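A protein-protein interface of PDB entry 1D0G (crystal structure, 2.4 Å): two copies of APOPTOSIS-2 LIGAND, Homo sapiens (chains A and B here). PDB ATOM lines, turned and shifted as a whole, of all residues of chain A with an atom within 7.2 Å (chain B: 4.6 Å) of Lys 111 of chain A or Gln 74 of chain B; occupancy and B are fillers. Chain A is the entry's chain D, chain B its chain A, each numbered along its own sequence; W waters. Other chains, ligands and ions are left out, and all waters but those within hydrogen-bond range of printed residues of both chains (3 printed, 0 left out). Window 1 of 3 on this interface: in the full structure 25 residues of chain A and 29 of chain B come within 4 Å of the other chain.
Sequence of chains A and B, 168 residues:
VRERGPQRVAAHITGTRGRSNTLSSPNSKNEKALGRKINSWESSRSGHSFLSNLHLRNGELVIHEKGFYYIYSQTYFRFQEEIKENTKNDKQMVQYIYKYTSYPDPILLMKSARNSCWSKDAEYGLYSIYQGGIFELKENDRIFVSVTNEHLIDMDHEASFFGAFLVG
Gln 74 of chain B touches just these residues of chain A: Lys 111, Ser 112 and Gln 131. Of the printed residues of chain B, Leu 108 of chain A touches Glu 158 (3.4 Å). Of the printed residues of chain A, Glu 158 of chain B touches Leu 108, Leu 109, Met 110 and Lys 111. Ile 97 of chain A touches none of the printed residues of chain B. Leu 34 of chain A touches none of the printed residues of chain B. The nearest printed residue of chain B that does not touch Lys 111 of chain A is Ser 128 of chain B (4.5 Å).
The side-chain hydroxyl (OG) of Ser 73 of chain B sits at hydrogen-bond distance from the backbone carbonyl oxygen (O) of Phe 161 of chain B, at 2.9 Å. N of Phe 161 of chain B lies within hydrogen-bond range of O of Gln 74 of chain B (2.9 Å). The backbone NH of Tyr 76 of chain B sits at hydrogen-bond distance from the side-chain hydroxyl of Ser 160 of chain B (3.0 Å). The side-chain amide nitrogen of Gln 95 of chain A lies close to the side-chain amide nitrogen of Gln 131 of chain A (3.0 Å). The backbone carbonyl oxygen (O) of Met 110 of chain A is in hydrogen-bond range of the side-chain amide nitrogen (NE2) of Gln 131 of chain A (3.5 Å). OE1 of Gln 131 of chain A sits close to N of Lys 111 of chain A, 3.1 Å away.
Tyr 130 of chain B touches its own counterpart, Tyr 130 of chain A. Of the 16 pairs that touch across the chains among the printed residues, 1 has its exchanged pair printed and touching as well.
Of the 15 printed residues of chain A, 9 touch a printed residue of chain B. Hydrophobic or aromatic side chains of chain A that line the printed part of chain B: Leu 108, Met 110, Ala 113 and Tyr 130. Of the 13 printed residues of chain B, 7 touch a printed residue of chain A. Hydrophobic or aromatic side chains of chain B within 4 Å of the printed part of chain A: Tyr 76, Tyr 130 and Phe 161. Along chain B the printed residues that touch a printed residue of chain A span positions 74 to 161.
Water W3 bridges the side-chain carboxylate of Asp 156 of chain B (2.7 Å) and the side-chain amino group of Lys 111 of chain A (2.8 Å). Water W1 lies within hydrogen-bond range of the backbone carbonyl oxygen (O) of Leu 108 of chain A (2.7 Å) and the side-chain carboxylate (OE2) of Glu 158 of chain B (2.9 Å). Water W2 lies within hydrogen-bond range of the backbone carbonyl oxygen (O) of Ala 159 of chain B (2.8 Å), the backbone carbonyl oxygen (O) of Lys 111 of chain A (2.9 Å), the side-chain hydroxyl (OG) of Ser 128 of chain B (2.9 Å) and the side-chain amide nitrogen (NE2) of Gln 74 of chain B (3.3 Å).
Among the printed residues, merely in contact across the chains: Gly 132 of chain A with Phe 161 of chain B, Ser 112 of chain A with Ser 128 of chain B, Gly 132 of chain A with Tyr 130 of chain B, Met 110 of chain A with Glu 158 of chain B, Leu 109 of chain A with Glu 158 of chain B, Tyr 130 of chain A with Tyr 130 of chain B, Leu 108 of chain A with Glu 158 of chain B, Met 110 of chain A with Phe 161 of chain B, Ala 113 of chain A with Tyr 76 of chain B, Lys 111 of chain A with Tyr 76 of chain B and Lys 111 of chain A with Ala 159 of chain B.
The side-chain amide nitrogen of Gln 74 of chain B is in hydrogen-bond range of the backbone carbonyl oxygen of Lys 111 of chain A, 3.1 Å away. The side-chain amide oxygen (OE1) of Gln 74 of chain B sits at hydrogen-bond distance from the side-chain hydroxyl (OG) of Ser 112 of chain A (3.4 Å). The side-chain amide oxygen (OE1) of Gln 131 of chain A is in hydrogen-bond range of the side-chain amide nitrogen (NE2) of Gln 74 of chain B (3.0 Å). The side-chain hydroxyl (OG) of Ser 128 of chain B lies within hydrogen-bond range of the backbone NH (N) of Ala 113 of chain A (2.8 Å). The backbone carbonyl oxygen of Glu 158 of chain B lies within hydrogen-bond range of the backbone NH of Lys 111 of chain A.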
ATOM      1  N   LEU A  34      26.926  -9.396   5.248  1.00  0.00           N
ATOM      2  CA  LEU A  34      25.543  -9.083   4.880  1.00  0.00           C
ATOM      3  C   LEU A  34      24.627  -9.243   6.119  1.00  0.00           C
ATOM      4  O   LEU A  34      24.982  -9.942   7.053  1.00  0.00           O
ATOM      5  CB  LEU A  34      25.098 -10.020   3.741  1.00  0.00           C
ATOM      6  CG  LEU A  34      25.922  -9.855   2.462  1.00  0.00           C
ATOM      7  CD1 LEU A  34      25.633 -10.919   1.450  1.00  0.00           C
ATOM      8  CD2 LEU A  34      25.630  -8.458   1.896  1.00  0.00           C
ATOM      9  N   VAL A  94      16.882 -13.938   4.900  1.00  0.00           N
ATOM     10  CA  VAL A  94      18.112 -14.649   4.623  1.00  0.00           C
ATOM     11  C   VAL A  94      18.960 -14.903   5.856  1.00  0.00           C
ATOM     12  O   VAL A  94      19.152 -14.013   6.691  1.00  0.00           O
ATOM     13  CB  VAL A  94      19.003 -13.854   3.620  1.00  0.00           C
ATOM     14  CG1 VAL A  94      20.110 -14.789   3.032  1.00  0.00           C
ATOM     15  CG2 VAL A  94      18.150 -13.231   2.519  1.00  0.00           C
ATOM     16  N   GLN A  95      19.479 -16.121   5.958  1.00  0.00           N
ATOM     17  CA  GLN A  95      20.360 -16.487   7.062  1.00  0.00           C
ATOM     18  C   GLN A  95      21.747 -16.696   6.450  1.00  0.00           C
ATOM     19  O   GLN A  95      21.875 -17.351   5.435  1.00  0.00           O
ATOM     20  CB  GLN A  95      19.904 -17.791   7.741  1.00  0.00           C
ATOM     21  CG  GLN A  95      20.776 -18.221   8.949  1.00  0.00           C
ATOM     22  CD  GLN A  95      20.634 -19.709   9.269  1.00  0.00           C
ATOM     23  OE1 GLN A  95      19.599 -20.154   9.759  1.00  0.00           O
ATOM     24  NE2 GLN A  95      21.655 -20.475   8.967  1.00  0.00           N
ATOM     25  N   TYR A  96      22.763 -16.107   7.056  1.00  0.00           N
ATOM     26  CA  TYR A  96      24.150 -16.223   6.603  1.00  0.00           C
ATOM     27  C   TYR A  96      25.001 -16.802   7.732  1.00  0.00           C
ATOM     28  O   TYR A  96      24.811 -16.461   8.897  1.00  0.00           O
ATOM     29  CB  TYR A  96      24.738 -14.849   6.234  1.00  0.00           C
ATOM     30  CG  TYR A  96      24.007 -14.065   5.156  1.00  0.00           C
ATOM     31  CD1 TYR A  96      24.207 -14.342   3.798  1.00  0.00           C
ATOM     32  CD2 TYR A  96      23.134 -13.029   5.496  1.00  0.00           C
ATOM     33  CE1 TYR A  96      23.553 -13.609   2.804  1.00  0.00           C
ATOM     34  CE2 TYR A  96      22.470 -12.278   4.506  1.00  0.00           C
ATOM     35  CZ  TYR A  96      22.680 -12.577   3.170  1.00  0.00           C
ATOM     36  OH  TYR A  96      21.989 -11.875   2.205  1.00  0.00           O
ATOM     37  N   ILE A  97      25.883 -17.738   7.399  1.00  0.00           N
ATOM     38  CA  ILE A  97      26.765 -18.289   8.421  1.00  0.00           C
ATOM     39  C   ILE A  97      28.178 -17.971   7.966  1.00  0.00           C
ATOM     40  O   ILE A  97      28.621 -18.480   6.929  1.00  0.00           O
ATOM     41  CB  ILE A  97      26.596 -19.806   8.591  1.00  0.00           C
ATOM     42  CG1 ILE A  97      25.210 -20.107   9.147  1.00  0.00           C
ATOM     43  CG2 ILE A  97      27.645 -20.322   9.536  1.00  0.00           C
ATOM     44  CD1 ILE A  97      24.831 -21.574   9.080  1.00  0.00           C
ATOM     45  N   LEU A 108      32.051 -15.830   4.025  1.00  0.00           N
ATOM     46  CA  LEU A 108      30.779 -16.521   4.057  1.00  0.00           C
ATOM     47  C   LEU A 108      30.901 -18.033   3.792  1.00  0.00           C
ATOM     48  O   LEU A 108      31.527 -18.465   2.826  1.00  0.00           O
ATOM     49  CB  LEU A 108      29.859 -15.887   3.022  1.00  0.00           C
ATOM     50  CG  LEU A 108      28.469 -16.498   2.845  1.00  0.00           C
ATOM     51  CD1 LEU A 108      27.547 -16.129   4.015  1.00  0.00           C
ATOM     52  CD2 LEU A 108      27.894 -16.001   1.508  1.00  0.00           C
ATOM     53  N   LEU A 109      30.303 -18.849   4.650  1.00  0.00           N
ATOM     54  CA  LEU A 109      30.344 -20.287   4.452  1.00  0.00           C
ATOM     55  C   LEU A 109      29.050 -20.744   3.798  1.00  0.00           C
ATOM     56  O   LEU A 109      29.054 -21.454   2.790  1.00  0.00           O
ATOM     57  CB  LEU A 109      30.492 -20.998   5.793  1.00  0.00           C
ATOM     58  CG  LEU A 109      31.705 -20.610   6.642  1.00  0.00           C
ATOM     59  CD1 LEU A 109      31.756 -21.514   7.914  1.00  0.00           C
ATOM     60  CD2 LEU A 109      32.982 -20.791   5.779  1.00  0.00           C
ATOM     61  N   MET A 110      27.933 -20.299   4.368  1.00  0.00           N
ATOM     62  CA  MET A 110      26.611 -20.720   3.892  1.00  0.00           C
ATOM     63  C   MET A 110      25.552 -19.623   3.935  1.00  0.00           C
ATOM     64  O   MET A 110      25.569 -18.754   4.813  1.00  0.00           O
ATOM     65  CB  MET A 110      26.105 -21.893   4.760  1.00  0.00           C
ATOM     66  CG  MET A 110      26.870 -23.221   4.664  1.00  0.00           C
ATOM     67  SD  MET A 110      26.346 -24.440   5.939  1.00  0.00           S
ATOM     68  CE  MET A 110      27.034 -23.806   7.459  1.00  0.00           C
ATOM     69  N   LYS A 111      24.616 -19.692   2.994  1.00  0.00           N
ATOM     70  CA  LYS A 111      23.500 -18.758   2.952  1.00  0.00           C
ATOM     71  C   LYS A 111      22.254 -19.497   2.485  1.00  0.00           C
ATOM     72  O   LYS A 111      22.313 -20.383   1.652  1.00  0.00           O
ATOM     73  CB  LYS A 111      23.790 -17.538   2.080  1.00  0.00           C
ATOM     74  CG  LYS A 111      23.262 -17.606   0.674  1.00  0.00           C
ATOM     75  CD  LYS A 111      23.655 -16.355  -0.095  1.00  0.00           C
ATOM     76  CE  LYS A 111      23.309 -16.504  -1.548  1.00  0.00           C
ATOM     77  NZ  LYS A 111      23.769 -15.265  -2.171  1.00  0.00           N
ATOM     78  N   SER A 112      21.128 -19.137   3.066  1.00  0.00           N
ATOM     79  CA  SER A 112      19.872 -19.777   2.758  1.00  0.00           C
ATOM     80  C   SER A 112      18.779 -18.698   2.795  1.00  0.00           C
ATOM     81  O   SER A 112      18.600 -18.027   3.815  1.00  0.00           O
ATOM     82  CB  SER A 112      19.633 -20.869   3.809  1.00  0.00           C
ATOM     83  OG  SER A 112      18.457 -21.593   3.561  1.00  0.00           O
ATOM     84  N   ALA A 113      18.018 -18.575   1.702  1.00  0.00           N
ATOM     85  CA  ALA A 113      16.997 -17.549   1.608  1.00  0.00           C
ATOM     86  C   ALA A 113      15.588 -17.969   1.249  1.00  0.00           C
ATOM     87  O   ALA A 113      15.351 -19.036   0.683  1.00  0.00           O
ATOM     88  CB  ALA A 113      17.468 -16.412   0.659  1.00  0.00           C
ATOM     89  N   ILE A 129      14.079 -21.121   8.895  1.00  0.00           N
ATOM     90  CA  ILE A 129      15.115 -21.432   7.934  1.00  0.00           C
ATOM     91  C   ILE A 129      16.209 -22.196   8.652  1.00  0.00           C
ATOM     92  O   ILE A 129      16.685 -21.765   9.669  1.00  0.00           O
ATOM     93  CB  ILE A 129      15.699 -20.108   7.325  1.00  0.00           C
ATOM     94  CG1 ILE A 129      14.621 -19.339   6.574  1.00  0.00           C
ATOM     95  CG2 ILE A 129      16.875 -20.381   6.419  1.00  0.00           C
ATOM     96  CD1 ILE A 129      15.165 -18.080   5.939  1.00  0.00           C
ATOM     97  N   TYR A 130      16.555 -23.358   8.121  1.00  0.00           N
ATOM     98  CA  TYR A 130      17.626 -24.193   8.656  1.00  0.00           C
ATOM     99  C   TYR A 130      18.591 -24.532   7.539  1.00  0.00           C
ATOM    100  O   TYR A 130      18.179 -24.809   6.419  1.00  0.00           O
ATOM    101  CB  TYR A 130      17.079 -25.520   9.183  1.00  0.00           C
ATOM    102  CG  TYR A 130      18.172 -26.504   9.572  1.00  0.00           C
ATOM    103  CD1 TYR A 130      18.846 -27.264   8.610  1.00  0.00           C
ATOM    104  CD2 TYR A 130      18.570 -26.628  10.916  1.00  0.00           C
ATOM    105  CE1 TYR A 130      19.886 -28.097   8.965  1.00  0.00           C
ATOM    106  CE2 TYR A 130      19.608 -27.459  11.280  1.00  0.00           C
ATOM    107  CZ  TYR A 130      20.272 -28.186  10.312  1.00  0.00           C
ATOM    108  OH  TYR A 130      21.368 -28.938  10.708  1.00  0.00           O
ATOM    109  N   GLN A 131      19.873 -24.567   7.857  1.00  0.00           N
ATOM    110  CA  GLN A 131      20.899 -24.964   6.878  1.00  0.00           C
ATOM    111  C   GLN A 131      22.099 -25.457   7.678  1.00  0.00           C
ATOM    112  O   GLN A 131      22.227 -25.183   8.869  1.00  0.00           O
ATOM    113  CB  GLN A 131      21.314 -23.816   5.916  1.00  0.00           C
ATOM    114  CG  GLN A 131      22.151 -22.715   6.569  1.00  0.00           C
ATOM    115  CD  GLN A 131      22.610 -21.577   5.616  1.00  0.00           C
ATOM    116  OE1 GLN A 131      22.832 -21.790   4.416  1.00  0.00           O
ATOM    117  NE2 GLN A 131      22.828 -20.375   6.196  1.00  0.00           N
ATOM    118  N   GLY A 132      22.973 -26.187   7.010  1.00  0.00           N
ATOM    119  CA  GLY A 132      24.145 -26.708   7.679  1.00  0.00           C
ATOM    120  C   GLY A 132      25.079 -27.323   6.674  1.00  0.00           C
ATOM    121  O   GLY A 132      24.663 -27.678   5.573  1.00  0.00           O
ATOM    122  N   SER B  73      22.273 -32.070   1.418  1.00  0.00           N
ATOM    123  CA  SER B  73      22.439 -31.185   0.285  1.00  0.00           C
ATOM    124  C   SER B  73      21.575 -29.927   0.382  1.00  0.00           C
ATOM    125  O   SER B  73      20.484 -29.940   0.952  1.00  0.00           O
ATOM    126  CB  SER B  73      22.131 -31.917  -1.014  1.00  0.00           C
ATOM    127  OG  SER B  73      22.363 -31.075  -2.129  1.00  0.00           O
ATOM    128  N   GLN B  74      22.131 -28.807  -0.047  1.00  0.00           N
ATOM    129  CA  GLN B  74      21.341 -27.580  -0.110  1.00  0.00           C
ATOM    130  C   GLN B  74      21.352 -27.166  -1.587  1.00  0.00           C
ATOM    131  O   GLN B  74      22.391 -27.235  -2.247  1.00  0.00           O
ATOM    132  CB  GLN B  74      21.919 -26.462   0.754  1.00  0.00           C
ATOM    133  CG  GLN B  74      21.112 -25.203   0.652  1.00  0.00           C
ATOM    134  CD  GLN B  74      21.166 -24.343   1.890  1.00  0.00           C
ATOM    135  OE1 GLN B  74      20.240 -24.364   2.692  1.00  0.00           O
ATOM    136  NE2 GLN B  74      22.187 -23.505   2.003  1.00  0.00           N
ATOM    137  N   THR B  75      20.173 -26.865  -2.126  1.00  0.00           N
ATOM    138  CA  THR B  75      20.046 -26.414  -3.522  1.00  0.00           C
ATOM    139  C   THR B  75      19.226 -25.116  -3.507  1.00  0.00           C
ATOM    140  O   THR B  75      18.091 -25.091  -3.031  1.00  0.00           O
ATOM    141  CB  THR B  75      19.352 -27.473  -4.416  1.00  0.00           C
ATOM    142  OG1 THR B  75      18.076 -27.839  -3.859  1.00  0.00           O
ATOM    143  CG2 THR B  75      20.238 -28.698  -4.591  1.00  0.00           C
ATOM    144  N   TYR B  76      19.821 -24.034  -3.996  1.00  0.00           N
ATOM    145  CA  TYR B  76      19.167 -22.717  -4.000  1.00  0.00           C
ATOM    146  C   TYR B  76      18.402 -22.417  -5.279  1.00  0.00           C
ATOM    147  O   TYR B  76      19.024 -22.204  -6.314  1.00  0.00           O
ATOM    148  CB  TYR B  76      20.245 -21.639  -3.796  1.00  0.00           C
ATOM    149  CG  TYR B  76      19.781 -20.189  -3.636  1.00  0.00           C
ATOM    150  CD1 TYR B  76      18.486 -19.877  -3.237  1.00  0.00           C
ATOM    151  CD2 TYR B  76      20.677 -19.139  -3.826  1.00  0.00           C
ATOM    152  CE1 TYR B  76      18.102 -18.555  -3.027  1.00  0.00           C
ATOM    153  CE2 TYR B  76      20.312 -17.831  -3.618  1.00  0.00           C
ATOM    154  CZ  TYR B  76      19.021 -17.531  -3.212  1.00  0.00           C
ATOM    155  OH  TYR B  76      18.679 -16.220  -2.922  1.00  0.00           O
ATOM    156  N   GLN B  95      14.232 -31.302  -4.648  1.00  0.00           N
ATOM    157  CA  GLN B  95      15.611 -31.787  -4.559  1.00  0.00           C
ATOM    158  C   GLN B  95      15.569 -33.294  -4.227  1.00  0.00           C
ATOM    159  O   GLN B  95      14.926 -33.717  -3.275  1.00  0.00           O
ATOM    160  CB  GLN B  95      16.415 -31.046  -3.486  1.00  0.00           C
ATOM    161  CG  GLN B  95      17.828 -31.592  -3.341  1.00  0.00           C
ATOM    162  CD  GLN B  95      18.476 -31.282  -2.005  1.00  0.00           C
ATOM    163  OE1 GLN B  95      18.749 -30.119  -1.684  1.00  0.00           O
ATOM    164  NE2 GLN B  95      18.751 -32.309  -1.231  1.00  0.00           N
ATOM    165  N   SER B 128      15.611 -21.686  -0.918  1.00  0.00           N
ATOM    166  CA  SER B 128      16.732 -22.547  -0.527  1.00  0.00           C
ATOM    167  C   SER B 128      16.134 -23.809   0.099  1.00  0.00           C
ATOM    168  O   SER B 128      15.339 -23.729   1.036  1.00  0.00           O
ATOM    169  CB  SER B 128      17.607 -21.891   0.507  1.00  0.00           C
ATOM    170  OG  SER B 128      18.162 -20.734  -0.015  1.00  0.00           O
ATOM    171  N   ILE B 129      16.508 -24.958  -0.446  1.00  0.00           N
ATOM    172  CA  ILE B 129      16.036 -26.240   0.036  1.00  0.00           C
ATOM    173  C   ILE B 129      17.187 -27.062   0.612  1.00  0.00           C
ATOM    174  O   ILE B 129      18.159 -27.361  -0.082  1.00  0.00           O
ATOM    175  CB  ILE B 129      15.400 -27.039  -1.117  1.00  0.00           C
ATOM    176  CG1 ILE B 129      14.082 -26.397  -1.516  1.00  0.00           C
ATOM    177  CG2 ILE B 129      15.201 -28.518  -0.705  1.00  0.00           C
ATOM    178  CD1 ILE B 129      13.399 -27.077  -2.673  1.00  0.00           C
ATOM    179  N   TYR B 130      17.045 -27.447   1.871  1.00  0.00           N
ATOM    180  CA  TYR B 130      18.027 -28.276   2.557  1.00  0.00           C
ATOM    181  C   TYR B 130      17.367 -29.554   3.112  1.00  0.00           C
ATOM    182  O   TYR B 130      16.247 -29.515   3.584  1.00  0.00           O
ATOM    183  CB  TYR B 130      18.647 -27.520   3.743  1.00  0.00           C
ATOM    184  CG  TYR B 130      19.590 -28.385   4.574  1.00  0.00           C
ATOM    185  CD1 TYR B 130      19.100 -29.280   5.537  1.00  0.00           C
ATOM    186  CD2 TYR B 130      20.985 -28.345   4.353  1.00  0.00           C
ATOM    187  CE1 TYR B 130      19.964 -30.109   6.237  1.00  0.00           C
ATOM    188  CE2 TYR B 130      21.854 -29.169   5.062  1.00  0.00           C
ATOM    189  CZ  TYR B 130      21.342 -30.048   5.999  1.00  0.00           C
ATOM    190  OH  TYR B 130      22.218 -30.859   6.700  1.00  0.00           O
ATOM    191  N   ASP B 156      26.288 -20.677  -6.581  1.00  0.00           N
ATOM    192  CA  ASP B 156      27.292 -20.057  -5.732  1.00  0.00           C
ATOM    193  C   ASP B 156      27.633 -21.085  -4.641  1.00  0.00           C
ATOM    194  O   ASP B 156      26.744 -21.712  -4.065  1.00  0.00           O
ATOM    195  CB  ASP B 156      26.744 -18.786  -5.107  1.00  0.00           C
ATOM    196  CG  ASP B 156      26.899 -17.568  -6.013  1.00  0.00           C
ATOM    197  OD1 ASP B 156      27.501 -17.670  -7.106  1.00  0.00           O
ATOM    198  OD2 ASP B 156      26.421 -16.492  -5.603  1.00  0.00           O
ATOM    199  N   GLU B 158      28.311 -21.002  -1.590  1.00  0.00           N
ATOM    200  CA  GLU B 158      27.728 -20.841  -0.269  1.00  0.00           C
ATOM    201  C   GLU B 158      26.254 -21.180  -0.255  1.00  0.00           C
ATOM    202  O   GLU B 158      25.676 -21.383   0.816  1.00  0.00           O
ATOM    203  CB  GLU B 158      27.858 -19.407   0.233  1.00  0.00           C
ATOM    204  CG  GLU B 158      29.265 -18.833   0.187  1.00  0.00           C
ATOM    205  CD  GLU B 158      29.564 -18.052  -1.097  1.00  0.00           C
ATOM    206  OE1 GLU B 158      28.939 -18.302  -2.149  1.00  0.00           O
ATOM    207  OE2 GLU B 158      30.452 -17.179  -1.039  1.00  0.00           O
ATOM    208  N   ALA B 159      25.659 -21.220  -1.444  1.00  0.00           N
ATOM    209  CA  ALA B 159      24.229 -21.442  -1.606  1.00  0.00           C
ATOM    210  C   ALA B 159      23.826 -22.850  -1.958  1.00  0.00           C
ATOM    211  O   ALA B 159      22.777 -23.316  -1.531  1.00  0.00           O
ATOM    212  CB  ALA B 159      23.673 -20.459  -2.666  1.00  0.00           C
ATOM    213  N   SER B 160      24.617 -23.501  -2.802  1.00  0.00           N
ATOM    214  CA  SER B 160      24.320 -24.872  -3.210  1.00  0.00           C
ATOM    215  C   SER B 160      25.527 -25.776  -2.938  1.00  0.00           C
ATOM    216  O   SER B 160      26.679 -25.462  -3.284  1.00  0.00           O
ATOM    217  CB  SER B 160      23.876 -24.928  -4.667  1.00  0.00           C
ATOM    218  OG  SER B 160      22.694 -24.161  -4.876  1.00  0.00           O
ATOM    219  N   PHE B 161      25.266 -26.879  -2.262  1.00  0.00           N
ATOM    220  CA  PHE B 161      26.314 -27.790  -1.896  1.00  0.00           C
ATOM    221  C   PHE B 161      25.807 -29.181  -1.622  1.00  0.00           C
ATOM    222  O   PHE B 161      24.615 -29.407  -1.445  1.00  0.00           O
ATOM    223  CB  PHE B 161      27.120 -27.222  -0.715  1.00  0.00           C
ATOM    224  CG  PHE B 161      26.276 -26.685   0.418  1.00  0.00           C
ATOM    225  CD1 PHE B 161      25.763 -27.550   1.390  1.00  0.00           C
ATOM    226  CD2 PHE B 161      26.062 -25.309   0.561  1.00  0.00           C
ATOM    227  CE1 PHE B 161      25.065 -27.064   2.498  1.00  0.00           C
ATOM    228  CE2 PHE B 161      25.377 -24.805   1.655  1.00  0.00           C
ATOM    229  CZ  PHE B 161      24.866 -25.685   2.640  1.00  0.00           C
HETATM  230  O   HOH W   1      32.615 -16.970   0.827  1.00  0.00           O
HETATM  231  O   HOH W   2      20.842 -21.674  -0.421  1.00  0.00           O
HETATM  232  O   HOH W   3      23.843 -16.357  -4.787  1.00  0.00           O
